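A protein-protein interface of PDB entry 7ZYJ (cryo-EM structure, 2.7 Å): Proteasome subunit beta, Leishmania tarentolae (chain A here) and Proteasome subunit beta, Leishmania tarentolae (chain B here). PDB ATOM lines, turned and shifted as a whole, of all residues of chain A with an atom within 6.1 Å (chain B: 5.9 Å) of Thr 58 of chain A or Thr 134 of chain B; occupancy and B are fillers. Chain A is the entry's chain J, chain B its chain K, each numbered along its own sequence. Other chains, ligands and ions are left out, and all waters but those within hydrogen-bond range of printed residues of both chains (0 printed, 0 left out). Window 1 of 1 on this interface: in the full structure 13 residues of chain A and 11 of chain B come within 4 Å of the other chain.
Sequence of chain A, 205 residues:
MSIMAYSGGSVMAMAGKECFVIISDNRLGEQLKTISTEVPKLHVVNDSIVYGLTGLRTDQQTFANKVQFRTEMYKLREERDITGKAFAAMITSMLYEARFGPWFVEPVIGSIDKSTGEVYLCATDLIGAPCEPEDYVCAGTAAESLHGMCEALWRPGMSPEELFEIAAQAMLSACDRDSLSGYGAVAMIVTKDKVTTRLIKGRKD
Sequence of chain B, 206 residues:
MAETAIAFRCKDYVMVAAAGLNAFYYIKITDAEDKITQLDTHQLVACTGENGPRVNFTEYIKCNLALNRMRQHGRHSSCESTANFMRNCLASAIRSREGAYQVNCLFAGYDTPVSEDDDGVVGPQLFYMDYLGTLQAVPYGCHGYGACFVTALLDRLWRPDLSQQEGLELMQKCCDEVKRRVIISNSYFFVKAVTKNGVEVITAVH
The backbone carbonyl oxygen of Gly 133 of chain B sits at hydrogen-bond distance from the side-chain hydroxyl of Thr 58 of chain A. The side-chain carboxylate of Glu 30 of chain A is in hydrogen-bond range of the side-chain hydroxyl of Tyr 128 of chain B, at 2.5 Å. The side-chain amide nitrogen (NE2) of Gln 61 of chain A is in hydrogen-bond range of the backbone carbonyl oxygen (O) of Leu 135 of chain B. O of Thr 58 of chain A lies within hydrogen-bond range of NH1 of Arg 87 of chain B. O of Leu 132 of chain B is in hydrogen-bond range of OG1 of Thr 58 of chain A, at 2.8 Å. NH2 of Arg 87 of chain B is in hydrogen-bond range of OG1 of Thr 62 of chain A (3.0 Å).
The backbone carbonyl oxygen (O) of Gln 136 of chain B sits at hydrogen-bond distance from the backbone NH (N) of Tyr 128 of chain B (2.8 Å). The side-chain amide oxygen (OE1) of Gln 60 of chain A lies within hydrogen-bond range of the guanidinium group (NH1) of Arg 57 of chain A, 3.3 Å away. NH1 of Arg 87 of chain B lies within hydrogen-bond range of O of Gly 133 of chain B (2.8 Å). The side-chain hydroxyl (OG) of Ser 7 of chain A lies within hydrogen-bond range of the backbone NH (N) of Arg 57 of chain A, at 3.1 Å. O of Thr 58 of chain A sits at hydrogen-bond distance from OG1 of Thr 62 of chain A.
Among the printed residues, merely in contact across the chains: Leu 28 of chain A with Gln 136 of chain B, Glu 30 of chain A with Asp 130 of chain B, Arg 57 of chain A with Thr 134 of chain B, Thr 58 of chain A with Ala 91 of chain B, Thr 58 of chain A with Thr 134 of chain B, Gln 61 of chain A with Arg 87 of chain B, Gln 61 of chain A with Gly 133 of chain B, Gln 61 of chain A with Thr 134 of chain B and Thr 62 of chain A with Ala 91 of chain B.
Of chain A, only Arg 57 (3.6 Å), Thr 58 (3.8 Å) and Gln 61 (3.7 Å) come within 4 Å of Thr 134 of chain B. Of the printed residues of chain B, Leu 28 of chain A touches Gln 136. Of the printed residues of chain A, Arg 87 of chain B touches Thr 58, Gln 61 and Thr 62. Printed residues of chain B within 4 Å of Glu 30 of chain A: Tyr 128 and Asp 130. Of the printed residues of chain A, Gln 136 of chain B touches Leu 28. Of the printed residues of chain B, Gln 61 of chain A touches Arg 87, Gly 133, Thr 134 and Leu 135. Met 129 of chain B touches none of the printed residues of chain A. Tyr 131 of chain B touches none of the printed residues of chain A. The nearest residue of chain B that does not touch Thr 58 of chain A is Ile 94 of chain B (4.3 Å).
Of the 13 printed residues of chain A, 6 touch a printed residue of chain B. Printed residues of chain A that touch a printed residue of chain B: Leu 28, Glu 30, Arg 57, Thr 58, Gln 61 and Thr 62. Hydrophobic or aromatic side chains of chain A that line the printed part of chain B: Leu 28. Along chain B the printed residues that touch a printed residue of chain A span positions 87 to 136. Among the printed residues, 15 pairs touch across the chains.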
ATOM      1  N   SER A   7      28.474 -26.754  19.864  1.00  0.00           N
ATOM      2  CA  SER A   7      27.456 -27.793  19.909  1.00  0.00           C
ATOM      3  C   SER A   7      26.743 -28.003  18.581  1.00  0.00           C
ATOM      4  O   SER A   7      26.038 -29.007  18.429  1.00  0.00           O
ATOM      5  CB  SER A   7      26.417 -27.470  20.988  1.00  0.00           C
ATOM      6  OG  SER A   7      27.023 -27.370  22.263  1.00  0.00           O
ATOM      7  N   LEU A  28      23.421 -33.036  17.743  1.00  0.00           N
ATOM      8  CA  LEU A  28      24.119 -32.484  18.898  1.00  0.00           C
ATOM      9  C   LEU A  28      25.504 -33.107  18.942  1.00  0.00           C
ATOM     10  O   LEU A  28      25.632 -34.336  18.932  1.00  0.00           O
ATOM     11  CB  LEU A  28      23.362 -32.759  20.198  1.00  0.00           C
ATOM     12  CG  LEU A  28      24.164 -32.529  21.480  1.00  0.00           C
ATOM     13  CD1 LEU A  28      24.368 -31.045  21.726  1.00  0.00           C
ATOM     14  CD2 LEU A  28      23.481 -33.182  22.668  1.00  0.00           C
ATOM     15  N   GLU A  30      30.103 -32.324  19.802  1.00  0.00           N
ATOM     16  CA  GLU A  30      31.168 -31.589  20.484  1.00  0.00           C
ATOM     17  C   GLU A  30      32.248 -31.247  19.460  1.00  0.00           C
ATOM     18  O   GLU A  30      33.273 -31.925  19.353  1.00  0.00           O
ATOM     19  CB  GLU A  30      31.725 -32.405  21.647  1.00  0.00           C
ATOM     20  CG  GLU A  30      30.972 -32.214  22.950  1.00  0.00           C
ATOM     21  CD  GLU A  30      31.242 -33.322  23.947  1.00  0.00           C
ATOM     22  OE1 GLU A  30      32.284 -33.998  23.818  1.00  0.00           O
ATOM     23  OE2 GLU A  30      30.414 -33.516  24.861  1.00  0.00           O
ATOM     24  N   GLY A  55      23.198 -22.579  20.007  1.00  0.00           N
ATOM     25  CA  GLY A  55      24.417 -22.137  20.651  1.00  0.00           C
ATOM     26  C   GLY A  55      25.007 -23.220  21.526  1.00  0.00           C
ATOM     27  O   GLY A  55      24.828 -24.408  21.245  1.00  0.00           O
ATOM     28  N   LEU A  56      25.722 -22.829  22.578  1.00  0.00           N
ATOM     29  CA  LEU A  56      26.223 -23.805  23.536  1.00  0.00           C
ATOM     30  C   LEU A  56      25.053 -24.554  24.161  1.00  0.00           C
ATOM     31  O   LEU A  56      24.101 -23.942  24.652  1.00  0.00           O
ATOM     32  CB  LEU A  56      27.051 -23.105  24.612  1.00  0.00           C
ATOM     33  CG  LEU A  56      27.992 -23.982  25.438  1.00  0.00           C
ATOM     34  CD1 LEU A  56      28.911 -24.785  24.533  1.00  0.00           C
ATOM     35  CD2 LEU A  56      28.797 -23.135  26.405  1.00  0.00           C
ATOM     36  N   ARG A  57      25.130 -25.888  24.146  1.00  0.00           N
ATOM     37  CA  ARG A  57      23.975 -26.698  24.521  1.00  0.00           C
ATOM     38  C   ARG A  57      23.617 -26.518  25.992  1.00  0.00           C
ATOM     39  O   ARG A  57      22.433 -26.469  26.344  1.00  0.00           O
ATOM     40  CB  ARG A  57      24.240 -28.169  24.205  1.00  0.00           C
ATOM     41  CG  ARG A  57      23.095 -29.095  24.575  1.00  0.00           C
ATOM     42  CD  ARG A  57      21.830 -28.743  23.816  1.00  0.00           C
ATOM     43  NE  ARG A  57      20.721 -29.612  24.184  1.00  0.00           N
ATOM     44  CZ  ARG A  57      19.447 -29.347  23.933  1.00  0.00           C
ATOM     45  NH1 ARG A  57      19.079 -28.241  23.311  1.00  0.00           N
ATOM     46  NH2 ARG A  57      18.516 -30.215  24.319  1.00  0.00           N
ATOM     47  N   THR A  58      24.623 -26.422  26.864  1.00  0.00           N
ATOM     48  CA  THR A  58      24.345 -26.166  28.273  1.00  0.00           C
ATOM     49  C   THR A  58      23.655 -24.820  28.459  1.00  0.00           C
ATOM     50  O   THR A  58      22.723 -24.697  29.263  1.00  0.00           O
ATOM     51  CB  THR A  58      25.636 -26.246  29.094  1.00  0.00           C
ATOM     52  OG1 THR A  58      25.353 -25.953  30.467  1.00  0.00           O
ATOM     53  CG2 THR A  58      26.691 -25.281  28.575  1.00  0.00           C
ATOM     54  N   ASP A  59      24.087 -23.801  27.712  1.00  0.00           N
ATOM     55  CA  ASP A  59      23.411 -22.511  27.767  1.00  0.00           C
ATOM     56  C   ASP A  59      22.005 -22.606  27.194  1.00  0.00           C
ATOM     57  O   ASP A  59      21.081 -21.968  27.707  1.00  0.00           O
ATOM     58  CB  ASP A  59      24.226 -21.452  27.030  1.00  0.00           C
ATOM     59  CG  ASP A  59      25.302 -20.839  27.900  1.00  0.00           C
ATOM     60  OD1 ASP A  59      25.605 -21.417  28.963  1.00  0.00           O
ATOM     61  OD2 ASP A  59      25.838 -19.777  27.526  1.00  0.00           O
ATOM     62  N   GLN A  60      21.823 -23.395  26.131  1.00  0.00           N
ATOM     63  CA  GLN A  60      20.483 -23.618  25.598  1.00  0.00           C
ATOM     64  C   GLN A  60      19.560 -24.178  26.669  1.00  0.00           C
ATOM     65  O   GLN A  60      18.445 -23.688  26.865  1.00  0.00           O
ATOM     66  CB  GLN A  60      20.536 -24.568  24.402  1.00  0.00           C
ATOM     67  CG  GLN A  60      21.311 -24.059  23.207  1.00  0.00           C
ATOM     68  CD  GLN A  60      21.298 -25.044  22.057  1.00  0.00           C
ATOM     69  OE1 GLN A  60      20.253 -25.586  21.704  1.00  0.00           O
ATOM     70  NE2 GLN A  60      22.463 -25.288  21.473  1.00  0.00           N
ATOM     71  N   GLN A  61      20.025 -25.199  27.389  1.00  0.00           N
ATOM     72  CA  GLN A  61      19.184 -25.843  28.390  1.00  0.00           C
ATOM     73  C   GLN A  61      18.922 -24.923  29.577  1.00  0.00           C
ATOM     74  O   GLN A  61      17.792 -24.849  30.074  1.00  0.00           O
ATOM     75  CB  GLN A  61      19.830 -27.152  28.838  1.00  0.00           C
ATOM     76  CG  GLN A  61      19.967 -28.167  27.712  1.00  0.00           C
ATOM     77  CD  GLN A  61      20.605 -29.465  28.160  1.00  0.00           C
ATOM     78  OE1 GLN A  61      21.771 -29.495  28.551  1.00  0.00           O
ATOM     79  NE2 GLN A  61      19.843 -30.548  28.100  1.00  0.00           N
ATOM     80  N   THR A  62      19.948 -24.200  30.038  1.00  0.00           N
ATOM     81  CA  THR A  62      19.762 -23.279  31.156  1.00  0.00           C
ATOM     82  C   THR A  62      18.789 -22.163  30.795  1.00  0.00           C
ATOM     83  O   THR A  62      17.888 -21.828  31.574  1.00  0.00           O
ATOM     84  CB  THR A  62      21.107 -22.699  31.588  1.00  0.00           C
ATOM     85  OG1 THR A  62      22.037 -23.765  31.818  1.00  0.00           O
ATOM     86  CG2 THR A  62      20.952 -21.888  32.862  1.00  0.00           C
ATOM     87  N   PHE A  63      18.949 -21.579  29.604  1.00  0.00           N
ATOM     88  CA  PHE A  63      18.051 -20.518  29.173  1.00  0.00           C
ATOM     89  C   PHE A  63      16.638 -21.035  28.950  1.00  0.00           C
ATOM     90  O   PHE A  63      15.673 -20.326  29.247  1.00  0.00           O
ATOM     91  CB  PHE A  63      18.588 -19.859  27.902  1.00  0.00           C
ATOM     92  CG  PHE A  63      17.937 -18.547  27.582  1.00  0.00           C
ATOM     93  CD1 PHE A  63      18.279 -17.402  28.280  1.00  0.00           C
ATOM     94  CD2 PHE A  63      16.981 -18.458  26.585  1.00  0.00           C
ATOM     95  CE1 PHE A  63      17.679 -16.193  27.991  1.00  0.00           C
ATOM     96  CE2 PHE A  63      16.379 -17.252  26.291  1.00  0.00           C
ATOM     97  CZ  PHE A  63      16.728 -16.118  26.994  1.00  0.00           C
ATOM     98  N   TRP A 103      24.738 -15.065  27.871  1.00  0.00           N
ATOM     99  CA  TRP A 103      24.382 -16.416  27.472  1.00  0.00           C
ATOM    100  C   TRP A 103      24.786 -16.637  26.021  1.00  0.00           C
ATOM    101  O   TRP A 103      24.811 -15.708  25.211  1.00  0.00           O
ATOM    102  CB  TRP A 103      22.881 -16.656  27.635  1.00  0.00           C
ATOM    103  CG  TRP A 103      22.374 -16.438  29.023  1.00  0.00           C
ATOM    104  CD1 TRP A 103      21.647 -15.376  29.474  1.00  0.00           C
ATOM    105  CD2 TRP A 103      22.547 -17.311  30.144  1.00  0.00           C
ATOM    106  NE1 TRP A 103      21.360 -15.530  30.807  1.00  0.00           N
ATOM    107  CE2 TRP A 103      21.902 -16.711  31.243  1.00  0.00           C
ATOM    108  CE3 TRP A 103      23.186 -18.540  30.327  1.00  0.00           C
ATOM    109  CZ2 TRP A 103      21.878 -17.297  32.505  1.00  0.00           C
ATOM    110  CZ3 TRP A 103      23.161 -19.121  31.580  1.00  0.00           C
ATOM    111  CH2 TRP A 103      22.512 -18.499  32.652  1.00  0.00           C
ATOM    112  N   ARG B  87      23.031 -31.677  36.369  1.00  0.00           N
ATOM    113  CA  ARG B  87      23.224 -30.742  35.269  1.00  0.00           C
ATOM    114  C   ARG B  87      23.153 -29.302  35.754  1.00  0.00           C
ATOM    115  O   ARG B  87      23.945 -28.458  35.325  1.00  0.00           O
ATOM    116  CB  ARG B  87      22.181 -30.989  34.182  1.00  0.00           C
ATOM    117  CG  ARG B  87      22.469 -30.262  32.891  1.00  0.00           C
ATOM    118  CD  ARG B  87      21.197 -29.790  32.218  1.00  0.00           C
ATOM    119  NE  ARG B  87      20.764 -28.499  32.736  1.00  0.00           N
ATOM    120  CZ  ARG B  87      21.269 -27.333  32.361  1.00  0.00           C
ATOM    121  NH1 ARG B  87      22.234 -27.256  31.459  1.00  0.00           N
ATOM    122  NH2 ARG B  87      20.797 -26.216  32.905  1.00  0.00           N
ATOM    123  N   LEU B  90      26.439 -28.529  37.585  1.00  0.00           N
ATOM    124  CA  LEU B  90      27.546 -28.328  36.655  1.00  0.00           C
ATOM    125  C   LEU B  90      27.408 -27.010  35.902  1.00  0.00           C
ATOM    126  O   LEU B  90      28.396 -26.295  35.704  1.00  0.00           O
ATOM    127  CB  LEU B  90      27.629 -29.498  35.676  1.00  0.00           C
ATOM    128  CG  LEU B  90      28.031 -30.849  36.270  1.00  0.00           C
ATOM    129  CD1 LEU B  90      27.623 -31.982  35.345  1.00  0.00           C
ATOM    130  CD2 LEU B  90      29.523 -30.891  36.552  1.00  0.00           C
ATOM    131  N   ALA B  91      26.190 -26.672  35.473  1.00  0.00           N
ATOM    132  CA  ALA B  91      25.975 -25.428  34.742  1.00  0.00           C
ATOM    133  C   ALA B  91      26.200 -24.214  35.633  1.00  0.00           C
ATOM    134  O   ALA B  91      26.737 -23.197  35.179  1.00  0.00           O
ATOM    135  CB  ALA B  91      24.568 -25.407  34.148  1.00  0.00           C
ATOM    136  N   ILE B  94      30.073 -23.377  36.019  1.00  0.00           N
ATOM    137  CA  ILE B  94      30.825 -22.739  34.940  1.00  0.00           C
ATOM    138  C   ILE B  94      30.705 -21.223  34.936  1.00  0.00           C
ATOM    139  O   ILE B  94      31.476 -20.556  34.237  1.00  0.00           O
ATOM    140  CB  ILE B  94      30.394 -23.272  33.558  1.00  0.00           C
ATOM    141  CG1 ILE B  94      29.085 -22.621  33.110  1.00  0.00           C
ATOM    142  CG2 ILE B  94      30.258 -24.783  33.581  1.00  0.00           C
ATOM    143  CD1 ILE B  94      28.666 -23.010  31.715  1.00  0.00           C
ATOM    144  N   TYR B 128      24.295 -38.802  29.223  1.00  0.00           N
ATOM    145  CA  TYR B 128      25.608 -38.236  28.959  1.00  0.00           C
ATOM    146  C   TYR B 128      25.665 -36.813  29.502  1.00  0.00           C
ATOM    147  O   TYR B 128      24.736 -36.023  29.298  1.00  0.00           O
ATOM    148  CB  TYR B 128      25.869 -38.252  27.449  1.00  0.00           C
ATOM    149  CG  TYR B 128      27.162 -37.627  26.978  1.00  0.00           C
ATOM    150  CD1 TYR B 128      27.256 -36.259  26.755  1.00  0.00           C
ATOM    151  CD2 TYR B 128      28.273 -38.411  26.706  1.00  0.00           C
ATOM    152  CE1 TYR B 128      28.429 -35.687  26.310  1.00  0.00           C
ATOM    153  CE2 TYR B 128      29.448 -37.849  26.254  1.00  0.00           C
ATOM    154  CZ  TYR B 128      29.521 -36.486  26.061  1.00  0.00           C
ATOM    155  OH  TYR B 128      30.692 -35.920  25.614  1.00  0.00           O
ATOM    156  N   MET B 129      26.763 -36.487  30.189  1.00  0.00           N
ATOM    157  CA  MET B 129      26.920 -35.192  30.842  1.00  0.00           C
ATOM    158  C   MET B 129      28.300 -34.636  30.533  1.00  0.00           C
ATOM    159  O   MET B 129      29.311 -35.240  30.911  1.00  0.00           O
ATOM    160  CB  MET B 129      26.743 -35.311  32.357  1.00  0.00           C
ATOM    161  CG  MET B 129      25.348 -35.668  32.818  1.00  0.00           C
ATOM    162  SD  MET B 129      25.286 -35.784  34.615  1.00  0.00           S
ATOM    163  CE  MET B 129      23.596 -36.303  34.864  1.00  0.00           C
ATOM    164  N   ASP B 130      28.338 -33.484  29.874  1.00  0.00           N
ATOM    165  CA  ASP B 130      29.579 -32.754  29.677  1.00  0.00           C
ATOM    166  C   ASP B 130      29.899 -31.919  30.913  1.00  0.00           C
ATOM    167  O   ASP B 130      29.028 -31.614  31.732  1.00  0.00           O
ATOM    168  CB  ASP B 130      29.484 -31.857  28.444  1.00  0.00           C
ATOM    169  CG  ASP B 130      30.838 -31.528  27.855  1.00  0.00           C
ATOM    170  OD1 ASP B 130      31.809 -32.253  28.151  1.00  0.00           O
ATOM    171  OD2 ASP B 130      30.932 -30.542  27.094  1.00  0.00           O
ATOM    172  N   TYR B 131      31.174 -31.547  31.042  1.00  0.00           N
ATOM    173  CA  TYR B 131      31.598 -30.742  32.182  1.00  0.00           C
ATOM    174  C   TYR B 131      30.994 -29.344  32.162  1.00  0.00           C
ATOM    175  O   TYR B 131      30.912 -28.705  33.215  1.00  0.00           O
ATOM    176  CB  TYR B 131      33.123 -30.644  32.223  1.00  0.00           C
ATOM    177  CG  TYR B 131      33.708 -29.702  31.199  1.00  0.00           C
ATOM    178  CD1 TYR B 131      33.749 -30.043  29.856  1.00  0.00           C
ATOM    179  CD2 TYR B 131      34.222 -28.470  31.578  1.00  0.00           C
ATOM    180  CE1 TYR B 131      34.282 -29.184  28.919  1.00  0.00           C
ATOM    181  CE2 TYR B 131      34.759 -27.605  30.647  1.00  0.00           C
ATOM    182  CZ  TYR B 131      34.784 -27.967  29.319  1.00  0.00           C
ATOM    183  OH  TYR B 131      35.318 -27.109  28.387  1.00  0.00           O
ATOM    184  N   LEU B 132      30.569 -28.859  30.995  1.00  0.00           N
ATOM    185  CA  LEU B 132      29.973 -27.534  30.895  1.00  0.00           C
ATOM    186  C   LEU B 132      28.524 -27.505  31.354  1.00  0.00           C
ATOM    187  O   LEU B 132      27.951 -26.418  31.485  1.00  0.00           O
ATOM    188  CB  LEU B 132      30.058 -27.026  29.455  1.00  0.00           C
ATOM    189  CG  LEU B 132      31.449 -26.644  28.952  1.00  0.00           C
ATOM    190  CD1 LEU B 132      31.389 -26.239  27.491  1.00  0.00           C
ATOM    191  CD2 LEU B 132      32.023 -25.522  29.799  1.00  0.00           C
ATOM    192  N   GLY B 133      27.924 -28.657  31.600  1.00  0.00           N
ATOM    193  CA  GLY B 133      26.529 -28.745  31.948  1.00  0.00           C
ATOM    194  C   GLY B 133      25.618 -29.253  30.852  1.00  0.00           C
ATOM    195  O   GLY B 133      24.418 -28.965  30.896  1.00  0.00           O
ATOM    196  N   THR B 134      26.146 -29.965  29.862  1.00  0.00           N
ATOM    197  CA  THR B 134      25.311 -30.599  28.855  1.00  0.00           C
ATOM    198  C   THR B 134      24.699 -31.873  29.420  1.00  0.00           C
ATOM    199  O   THR B 134      25.348 -32.611  30.163  1.00  0.00           O
ATOM    200  CB  THR B 134      26.129 -30.920  27.604  1.00  0.00           C
ATOM    201  OG1 THR B 134      26.918 -29.780  27.240  1.00  0.00           O
ATOM    202  CG2 THR B 134      25.221 -31.296  26.445  1.00  0.00           C
ATOM    203  N   LEU B 135      23.440 -32.121  29.075  1.00  0.00           N
ATOM    204  CA  LEU B 135      22.742 -33.327  29.505  1.00  0.00           C
ATOM    205  C   LEU B 135      21.982 -33.892  28.318  1.00  0.00           C
ATOM    206  O   LEU B 135      21.212 -33.172  27.678  1.00  0.00           O
ATOM    207  CB  LEU B 135      21.787 -33.034  30.663  1.00  0.00           C
ATOM    208  CG  LEU B 135      20.922 -34.207  31.122  1.00  0.00           C
ATOM    209  CD1 LEU B 135      21.700 -35.093  32.070  1.00  0.00           C
ATOM    210  CD2 LEU B 135      19.645 -33.707  31.776  1.00  0.00           C
ATOM    211  N   GLN B 136      22.194 -35.173  28.025  1.00  0.00           N
ATOM    212  CA  GLN B 136      21.499 -35.787  26.901  1.00  0.00           C
ATOM    213  C   GLN B 136      21.218 -37.252  27.191  1.00  0.00           C
ATOM    214  O   GLN B 136      22.123 -37.995  27.572  1.00  0.00           O
ATOM    215  CB  GLN B 136      22.317 -35.651  25.611  1.00  0.00           C
ATOM    216  CG  GLN B 136      21.692 -36.329  24.404  1.00  0.00           C
ATOM    217  CD  GLN B 136      20.300 -35.817  24.098  1.00  0.00           C
ATOM    218  OE1 GLN B 136      19.404 -36.589  23.756  1.00  0.00           O
ATOM    219  NE2 GLN B 136      20.111 -34.509  24.212  1.00  0.00           N
